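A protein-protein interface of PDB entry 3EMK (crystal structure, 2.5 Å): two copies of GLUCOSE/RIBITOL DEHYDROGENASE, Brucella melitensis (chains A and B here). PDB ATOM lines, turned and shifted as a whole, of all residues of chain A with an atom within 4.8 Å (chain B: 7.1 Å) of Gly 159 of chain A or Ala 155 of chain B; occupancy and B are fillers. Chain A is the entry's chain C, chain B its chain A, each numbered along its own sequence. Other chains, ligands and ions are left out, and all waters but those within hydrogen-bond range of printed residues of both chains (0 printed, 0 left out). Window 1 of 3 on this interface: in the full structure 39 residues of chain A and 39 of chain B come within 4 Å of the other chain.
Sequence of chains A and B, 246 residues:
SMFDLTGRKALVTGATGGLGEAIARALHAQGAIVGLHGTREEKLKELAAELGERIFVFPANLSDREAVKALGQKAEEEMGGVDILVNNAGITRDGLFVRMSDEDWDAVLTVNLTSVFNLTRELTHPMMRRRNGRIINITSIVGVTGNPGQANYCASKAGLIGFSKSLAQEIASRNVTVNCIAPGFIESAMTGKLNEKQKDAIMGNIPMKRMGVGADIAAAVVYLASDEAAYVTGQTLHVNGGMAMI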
ATOM      1  N   LEU A 113      25.383   3.130  -6.111  1.00  0.00           N
ATOM      2  CA  LEU A 113      24.176   3.537  -5.439  1.00  0.00           C
ATOM      3  C   LEU A 113      23.142   2.413  -5.481  1.00  0.00           C
ATOM      4  O   LEU A 113      22.849   1.814  -4.457  1.00  0.00           O
ATOM      5  CB  LEU A 113      23.648   4.821  -6.069  1.00  0.00           C
ATOM      6  CG  LEU A 113      22.690   5.691  -5.258  1.00  0.00           C
ATOM      7  CD1 LEU A 113      23.329   6.154  -3.966  1.00  0.00           C
ATOM      8  CD2 LEU A 113      22.229   6.874  -6.080  1.00  0.00           C
ATOM      9  N   CYS A 154      30.286  11.876  -8.101  1.00  0.00           N
ATOM     10  CA  CYS A 154      29.943  12.787  -7.020  1.00  0.00           C
ATOM     11  C   CYS A 154      28.478  12.633  -6.658  1.00  0.00           C
ATOM     12  O   CYS A 154      28.118  12.640  -5.485  1.00  0.00           O
ATOM     13  CB  CYS A 154      30.257  14.222  -7.408  1.00  0.00           C
ATOM     14  SG  CYS A 154      31.996  14.635  -7.308  1.00  0.00           S
ATOM     15  N   ALA A 155      27.642  12.493  -7.678  1.00  0.00           N
ATOM     16  CA  ALA A 155      26.204  12.259  -7.487  1.00  0.00           C
ATOM     17  C   ALA A 155      25.903  10.982  -6.706  1.00  0.00           C
ATOM     18  O   ALA A 155      25.049  10.981  -5.812  1.00  0.00           O
ATOM     19  CB  ALA A 155      25.478  12.223  -8.843  1.00  0.00           C
ATOM     20  N   SER A 156      26.611   9.911  -7.049  1.00  0.00           N
ATOM     21  CA  SER A 156      26.399   8.614  -6.431  1.00  0.00           C
ATOM     22  C   SER A 156      26.872   8.654  -4.987  1.00  0.00           C
ATOM     23  O   SER A 156      26.182   8.199  -4.078  1.00  0.00           O
ATOM     24  CB  SER A 156      27.133   7.520  -7.205  1.00  0.00           C
ATOM     25  OG  SER A 156      28.530   7.529  -6.941  1.00  0.00           O
ATOM     26  N   LYS A 157      28.053   9.220  -4.778  1.00  0.00           N
ATOM     27  CA  LYS A 157      28.608   9.265  -3.443  1.00  0.00           C
ATOM     28  C   LYS A 157      27.801  10.168  -2.513  1.00  0.00           C
ATOM     29  O   LYS A 157      27.585   9.811  -1.343  1.00  0.00           O
ATOM     30  CB  LYS A 157      30.097   9.622  -3.484  1.00  0.00           C
ATOM     31  CG  LYS A 157      30.962   8.507  -4.051  1.00  0.00           C
ATOM     32  CD  LYS A 157      30.716   7.177  -3.324  1.00  0.00           C
ATOM     33  CE  LYS A 157      31.674   6.066  -3.752  1.00  0.00           C
ATOM     34  NZ  LYS A 157      31.334   4.832  -3.006  1.00  0.00           N
ATOM     35  N   ALA A 158      27.335  11.310  -3.034  1.00  0.00           N
ATOM     36  CA  ALA A 158      26.430  12.197  -2.270  1.00  0.00           C
ATOM     37  C   ALA A 158      25.133  11.463  -1.983  1.00  0.00           C
ATOM     38  O   ALA A 158      24.649  11.464  -0.858  1.00  0.00           O
ATOM     39  CB  ALA A 158      26.146  13.483  -3.022  1.00  0.00           C
ATOM     40  N   GLY A 159      24.587  10.823  -3.015  1.00  0.00           N
ATOM     41  CA  GLY A 159      23.368  10.027  -2.893  1.00  0.00           C
ATOM     42  C   GLY A 159      23.492   8.990  -1.807  1.00  0.00           C
ATOM     43  O   GLY A 159      22.557   8.792  -1.020  1.00  0.00           O
ATOM     44  N   LEU A 160      24.665   8.360  -1.744  1.00  0.00           N
ATOM     45  CA  LEU A 160      24.969   7.354  -0.742  1.00  0.00           C
ATOM     46  C   LEU A 160      24.816   7.835   0.699  1.00  0.00           C
ATOM     47  O   LEU A 160      24.324   7.090   1.556  1.00  0.00           O
ATOM     48  CB  LEU A 160      26.367   6.773  -0.959  1.00  0.00           C
ATOM     49  CG  LEU A 160      26.687   5.513  -0.150  1.00  0.00           C
ATOM     50  CD1 LEU A 160      25.827   4.328  -0.560  1.00  0.00           C
ATOM     51  CD2 LEU A 160      28.124   5.172  -0.317  1.00  0.00           C
ATOM     52  N   ILE A 161      25.220   9.073   0.967  1.00  0.00           N
ATOM     53  CA  ILE A 161      25.058   9.659   2.300  1.00  0.00           C
ATOM     54  C   ILE A 161      23.561   9.889   2.614  1.00  0.00           C
ATOM     55  O   ILE A 161      23.072   9.506   3.691  1.00  0.00           O
ATOM     56  CB  ILE A 161      25.881  10.971   2.474  1.00  0.00           C
ATOM     57  CG1 ILE A 161      27.377  10.671   2.379  1.00  0.00           C
ATOM     58  CG2 ILE A 161      25.526  11.663   3.808  1.00  0.00           C
ATOM     59  CD1 ILE A 161      28.267  11.889   2.101  1.00  0.00           C
ATOM     60  N   GLY A 162      22.854  10.510   1.667  1.00  0.00           N
ATOM     61  CA  GLY A 162      21.434  10.802   1.811  1.00  0.00           C
ATOM     62  C   GLY A 162      20.611   9.562   2.105  1.00  0.00           C
ATOM     63  O   GLY A 162      19.720   9.589   2.961  1.00  0.00           O
ATOM     64  N   PHE A 163      20.920   8.478   1.394  1.00  0.00           N
ATOM     65  CA  PHE A 163      20.273   7.201   1.570  1.00  0.00           C
ATOM     66  C   PHE A 163      20.538   6.681   2.961  1.00  0.00           C
ATOM     67  O   PHE A 163      19.608   6.249   3.662  1.00  0.00           O
ATOM     68  CB  PHE A 163      20.810   6.227   0.520  1.00  0.00           C
ATOM     69  CG  PHE A 163      20.558   4.764   0.826  1.00  0.00           C
ATOM     70  CD1 PHE A 163      19.291   4.216   0.698  1.00  0.00           C
ATOM     71  CD2 PHE A 163      21.607   3.930   1.191  1.00  0.00           C
ATOM     72  CE1 PHE A 163      19.073   2.859   0.953  1.00  0.00           C
ATOM     73  CE2 PHE A 163      21.406   2.573   1.442  1.00  0.00           C
ATOM     74  CZ  PHE A 163      20.143   2.034   1.325  1.00  0.00           C
ATOM     75  N   TRP B 105      12.456   2.389  -6.248  1.00  0.00           N
ATOM     76  CA  TRP B 105      13.776   2.983  -6.153  1.00  0.00           C
ATOM     77  C   TRP B 105      14.115   3.516  -7.542  1.00  0.00           C
ATOM     78  O   TRP B 105      14.338   4.736  -7.712  1.00  0.00           O
ATOM     79  CB  TRP B 105      14.792   1.947  -5.643  1.00  0.00           C
ATOM     80  CG  TRP B 105      16.198   2.385  -5.749  1.00  0.00           C
ATOM     81  CD1 TRP B 105      17.027   2.195  -6.815  1.00  0.00           C
ATOM     82  CD2 TRP B 105      16.959   3.115  -4.773  1.00  0.00           C
ATOM     83  NE1 TRP B 105      18.253   2.755  -6.566  1.00  0.00           N
ATOM     84  CE2 TRP B 105      18.241   3.332  -5.324  1.00  0.00           C
ATOM     85  CE3 TRP B 105      16.684   3.606  -3.485  1.00  0.00           C
ATOM     86  CZ2 TRP B 105      19.257   4.020  -4.629  1.00  0.00           C
ATOM     87  CZ3 TRP B 105      17.693   4.290  -2.793  1.00  0.00           C
ATOM     88  CH2 TRP B 105      18.959   4.492  -3.371  1.00  0.00           C
ATOM     89  N   VAL B 108      12.219   6.793  -8.950  1.00  0.00           N
ATOM     90  CA  VAL B 108      12.695   7.978  -8.225  1.00  0.00           C
ATOM     91  C   VAL B 108      14.088   8.439  -8.679  1.00  0.00           C
ATOM     92  O   VAL B 108      14.313   9.634  -8.858  1.00  0.00           O
ATOM     93  CB  VAL B 108      12.655   7.740  -6.694  1.00  0.00           C
ATOM     94  CG1 VAL B 108      13.457   8.807  -5.922  1.00  0.00           C
ATOM     95  CG2 VAL B 108      11.197   7.661  -6.217  1.00  0.00           C
ATOM     96  N   LEU B 109      15.004   7.493  -8.873  1.00  0.00           N
ATOM     97  CA  LEU B 109      16.353   7.809  -9.344  1.00  0.00           C
ATOM     98  C   LEU B 109      16.293   8.327 -10.757  1.00  0.00           C
ATOM     99  O   LEU B 109      16.792   9.427 -11.061  1.00  0.00           O
ATOM    100  CB  LEU B 109      17.265   6.583  -9.289  1.00  0.00           C
ATOM    101  CG  LEU B 109      18.095   6.459  -8.018  1.00  0.00           C
ATOM    102  CD1 LEU B 109      19.175   7.540  -8.005  1.00  0.00           C
ATOM    103  CD2 LEU B 109      17.210   6.586  -6.761  1.00  0.00           C
ATOM    104  N   LEU B 113      16.885  12.308 -10.552  1.00  0.00           N
ATOM    105  CA  LEU B 113      18.329  12.420 -10.711  1.00  0.00           C
ATOM    106  C   LEU B 113      18.770  12.318 -12.159  1.00  0.00           C
ATOM    107  O   LEU B 113      19.335  13.272 -12.704  1.00  0.00           O
ATOM    108  CB  LEU B 113      19.038  11.358  -9.863  1.00  0.00           C
ATOM    109  CG  LEU B 113      20.504  11.556  -9.490  1.00  0.00           C
ATOM    110  CD1 LEU B 113      20.847  13.012  -9.069  1.00  0.00           C
ATOM    111  CD2 LEU B 113      20.900  10.534  -8.421  1.00  0.00           C
ATOM    112  N   VAL B 142      15.244  17.433   3.068  1.00  0.00           N
ATOM    113  CA  VAL B 142      15.347  16.016   3.318  1.00  0.00           C
ATOM    114  C   VAL B 142      16.614  15.348   2.741  1.00  0.00           C
ATOM    115  O   VAL B 142      17.102  14.366   3.295  1.00  0.00           O
ATOM    116  CB  VAL B 142      14.027  15.384   2.815  1.00  0.00           C
ATOM    117  CG1 VAL B 142      14.248  14.213   1.856  1.00  0.00           C
ATOM    118  CG2 VAL B 142      13.083  15.113   3.997  1.00  0.00           C
ATOM    119  N   GLY B 143      17.153  15.901   1.653  1.00  0.00           N
ATOM    120  CA  GLY B 143      18.428  15.443   1.075  1.00  0.00           C
ATOM    121  C   GLY B 143      19.644  15.730   1.959  1.00  0.00           C
ATOM    122  O   GLY B 143      20.639  15.022   1.918  1.00  0.00           O
ATOM    123  N   GLN B 150      11.686   7.602   3.001  1.00  0.00           N
ATOM    124  CA  GLN B 150      12.106   8.216   1.744  1.00  0.00           C
ATOM    125  C   GLN B 150      13.555   7.935   1.416  1.00  0.00           C
ATOM    126  O   GLN B 150      14.255   8.827   0.932  1.00  0.00           O
ATOM    127  CB  GLN B 150      11.905   9.740   1.800  1.00  0.00           C
ATOM    128  CG  GLN B 150      10.494  10.226   2.145  1.00  0.00           C
ATOM    129  CD  GLN B 150      10.311  11.697   1.820  1.00  0.00           C
ATOM    130  OE1 GLN B 150      10.682  12.589   2.605  1.00  0.00           O
ATOM    131  NE2 GLN B 150       9.759  11.961   0.650  1.00  0.00           N
ATOM    132  N   ALA B 151      14.005   6.706   1.674  1.00  0.00           N
ATOM    133  CA  ALA B 151      15.381   6.312   1.387  1.00  0.00           C
ATOM    134  C   ALA B 151      15.744   6.679  -0.048  1.00  0.00           C
ATOM    135  O   ALA B 151      16.760   7.339  -0.289  1.00  0.00           O
ATOM    136  CB  ALA B 151      15.579   4.828   1.638  1.00  0.00           C
ATOM    137  N   ASN B 152      14.889   6.270  -0.987  1.00  0.00           N
ATOM    138  CA  ASN B 152      15.033   6.619  -2.404  1.00  0.00           C
ATOM    139  C   ASN B 152      15.023   8.122  -2.708  1.00  0.00           C
ATOM    140  O   ASN B 152      15.882   8.601  -3.437  1.00  0.00           O
ATOM    141  CB  ASN B 152      13.978   5.891  -3.269  1.00  0.00           C
ATOM    142  CG  ASN B 152      12.512   6.169  -2.832  1.00  0.00           C
ATOM    143  OD1 ASN B 152      12.242   6.864  -1.850  1.00  0.00           O
ATOM    144  ND2 ASN B 152      11.569   5.593  -3.576  1.00  0.00           N
ATOM    145  N   TYR B 153      14.056   8.856  -2.153  1.00  0.00           N
ATOM    146  CA  TYR B 153      13.929  10.292  -2.406  1.00  0.00           C
ATOM    147  C   TYR B 153      15.152  11.039  -1.883  1.00  0.00           C
ATOM    148  O   TYR B 153      15.723  11.861  -2.605  1.00  0.00           O
ATOM    149  CB  TYR B 153      12.622  10.832  -1.792  1.00  0.00           C
ATOM    150  CG  TYR B 153      12.312  12.275  -2.110  1.00  0.00           C
ATOM    151  CD1 TYR B 153      11.902  12.660  -3.384  1.00  0.00           C
ATOM    152  CD2 TYR B 153      12.404  13.267  -1.124  1.00  0.00           C
ATOM    153  CE1 TYR B 153      11.594  14.014  -3.682  1.00  0.00           C
ATOM    154  CE2 TYR B 153      12.108  14.625  -1.406  1.00  0.00           C
ATOM    155  CZ  TYR B 153      11.707  14.986  -2.688  1.00  0.00           C
ATOM    156  OH  TYR B 153      11.430  16.310  -2.981  1.00  0.00           O
ATOM    157  N   CYS B 154      15.573  10.728  -0.648  1.00  0.00           N
ATOM    158  CA  CYS B 154      16.713  11.400  -0.006  1.00  0.00           C
ATOM    159  C   CYS B 154      18.005  11.181  -0.760  1.00  0.00           C
ATOM    160  O   CYS B 154      18.825  12.099  -0.869  1.00  0.00           O
ATOM    161  CB  CYS B 154      16.890  10.945   1.444  1.00  0.00           C
ATOM    162  SG  CYS B 154      15.496  11.347   2.504  1.00  0.00           S
ATOM    163  N   ALA B 155      18.173   9.959  -1.277  1.00  0.00           N
ATOM    164  CA  ALA B 155      19.325   9.598  -2.094  1.00  0.00           C
ATOM    165  C   ALA B 155      19.318  10.433  -3.358  1.00  0.00           C
ATOM    166  O   ALA B 155      20.357  10.975  -3.802  1.00  0.00           O
ATOM    167  CB  ALA B 155      19.282   8.130  -2.438  1.00  0.00           C
ATOM    168  N   SER B 156      18.134  10.534  -3.946  1.00  0.00           N
ATOM    169  CA  SER B 156      18.008  11.228  -5.203  1.00  0.00           C
ATOM    170  C   SER B 156      18.264  12.711  -4.986  1.00  0.00           C
ATOM    171  O   SER B 156      18.850  13.362  -5.835  1.00  0.00           O
ATOM    172  CB  SER B 156      16.643  10.956  -5.838  1.00  0.00           C
ATOM    173  OG  SER B 156      15.641  11.811  -5.329  1.00  0.00           O
ATOM    174  N   LYS B 157      17.868  13.234  -3.831  1.00  0.00           N
ATOM    175  CA  LYS B 157      18.024  14.662  -3.562  1.00  0.00           C
ATOM    176  C   LYS B 157      19.399  15.075  -2.978  1.00  0.00           C
ATOM    177  O   LYS B 157      19.898  16.196  -3.251  1.00  0.00           O
ATOM    178  CB  LYS B 157      16.860  15.180  -2.701  1.00  0.00           C
ATOM    179  CG  LYS B 157      15.495  15.197  -3.416  1.00  0.00           C
ATOM    180  CD  LYS B 157      15.467  16.178  -4.567  1.00  0.00           C
ATOM    181  CE  LYS B 157      14.051  16.564  -4.923  1.00  0.00           C
ATOM    182  NZ  LYS B 157      14.021  17.256  -6.248  1.00  0.00           N
ATOM    183  N   ALA B 158      20.004  14.203  -2.170  1.00  0.00           N
ATOM    184  CA  ALA B 158      21.400  14.399  -1.781  1.00  0.00           C
ATOM    185  C   ALA B 158      22.322  14.326  -3.017  1.00  0.00           C
ATOM    186  O   ALA B 158      23.216  15.165  -3.174  1.00  0.00           O
ATOM    187  CB  ALA B 158      21.817  13.389  -0.740  1.00  0.00           C
ATOM    188  N   GLY B 159      22.089  13.329  -3.880  1.00  0.00           N
ATOM    189  CA  GLY B 159      22.853  13.135  -5.117  1.00  0.00           C
ATOM    190  C   GLY B 159      22.775  14.340  -6.037  1.00  0.00           C
ATOM    191  O   GLY B 159      23.790  14.763  -6.640  1.00  0.00           O
ATOM    192  N   LEU B 160      21.569  14.896  -6.142  1.00  0.00           N
ATOM    193  CA  LEU B 160      21.333  16.129  -6.864  1.00  0.00           C
ATOM    194  C   LEU B 160      22.277  17.230  -6.394  1.00  0.00           C
ATOM    195  O   LEU B 160      22.794  18.004  -7.207  1.00  0.00           O
ATOM    196  CB  LEU B 160      19.872  16.564  -6.676  1.00  0.00           C
ATOM    197  CG  LEU B 160      19.318  17.753  -7.482  1.00  0.00           C
ATOM    198  CD1 LEU B 160      19.530  17.560  -8.964  1.00  0.00           C
ATOM    199  CD2 LEU B 160      17.829  18.025  -7.178  1.00  0.00           C
ATOM    200  N   ILE B 161      22.511  17.310  -5.092  1.00  0.00           N
ATOM    201  CA  ILE B 161      23.406  18.350  -4.563  1.00  0.00           C
ATOM    202  C   ILE B 161      24.877  18.123  -4.976  1.00  0.00           C
ATOM    203  O   ILE B 161      25.586  19.065  -5.332  1.00  0.00           O
ATOM    204  CB  ILE B 161      23.245  18.491  -3.031  1.00  0.00           C
ATOM    205  CG1 ILE B 161      21.812  18.944  -2.709  1.00  0.00           C
ATOM    206  CG2 ILE B 161      24.329  19.435  -2.431  1.00  0.00           C
ATOM    207  CD1 ILE B 161      21.416  18.810  -1.284  1.00  0.00           C
ATOM    208  N   GLY B 162      25.313  16.867  -4.963  1.00  0.00           N
ATOM    209  CA  GLY B 162      26.699  16.520  -5.264  1.00  0.00           C
ATOM    210  C   GLY B 162      26.996  16.527  -6.744  1.00  0.00           C
ATOM    211  O   GLY B 162      28.130  16.702  -7.152  1.00  0.00           O
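The side-chain sulfur of Cys 154 of chain B lies within hydrogen-bond range of the backbone carbonyl oxygen of Gln 150 of chain B (3.2 Å).
O of Val 142 of chain B sits close to SG of Cys 154 of chain B.
Among the printed residues, pairs that only touch across the chains: Leu 113 of chain A with Trp 105 of chain B (3.9 Å), Leu 113 of chain A with Leu 109 of chain B (3.7 Å), Cys 154 of chain A with Gly 162 of chain B (3.3 Å), Ala 155 of chain A with Gly 159 of chain B (3.2 Å), Ala 158 of chain A with Ala 158 of chain B (3.4 Å), Ala 158 of chain A with Gly 159 of chain B (3.9 Å), Ala 158 of chain A with Gly 162 of chain B (3.8 Å), Gly 159 of chain A with Ala 155 of chain B (3.3 Å), Gly 159 of chain A with Gly 159 of chain B (3.6 Å), Gly 162 of chain A with Cys 154 of chain B (3.5 Å), Gly 162 of chain A with Ala 158 of chain B (3.7 Å), Phe 163 of chain A with Trp 105 of chain B (3.8 Å), Phe 163 of chain A with Ala 151 of chain B (3.9 Å) and Phe 163 of chain A with Ala 155 of chain B (3.8 Å).
Of the printed residues of chain A, Leu 109 of chain B touches Leu 113 (3.7 Å).
Ala 155 of chain B touches just these residues of chain A: Gly 159 (3.3 Å) and Phe 163 (3.8 Å).
Of the printed residues of chain A, Ala 158 of chain B touches Ala 158 (3.4 Å) and Gly 162 (3.7 Å).
Hydrophobic or aromatic side chains of chain A within 4 Å of the printed part of chain B: Leu 113, Ala 155, Ala 158 and Phe 163.
Printed residues of chain B that touch a printed residue of chain A: Trp 105, Leu 109, Ala 151, Cys 154, Ala 155, Ala 158, Gly 159 and Gly 162.
Hydrophobic or aromatic side chains of chain B that line the printed part of chain A: Trp 105, Leu 109, Ala 151, Ala 155 and Ala 158.
Among the printed residues, 14 pairs touch across the chains.
Among the printed residues, no Asp or Glu carboxylate lies within 4 Å of a Lys or Arg side-chain nitrogen of the other chain.
Ala 155 of chain A touches Gly 159 of chain B, and with the chains exchanged Gly 159 of chain A touches Ala 155 of chain B.
Ala 158 of chain B touches its own counterpart, Ala 158 of chain A.
Ala 158 of chain A touches Gly 159 of chain B, but with the chains exchanged Gly 159 of chain A does not touch Ala 158 of chain B (4.2 Å).
Ala 158 of chain A touches Gly 162 of chain B, and with the chains exchanged Gly 162 of chain A touches Ala 158 of chain B.
Positions printed for both chains: 113, 154, 155, 156, 157, 158, 159, 160, 161 and 162.
Of the 14 pairs that touch across the chains among the printed residues, 8 have their exchanged pair printed and touching as well.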
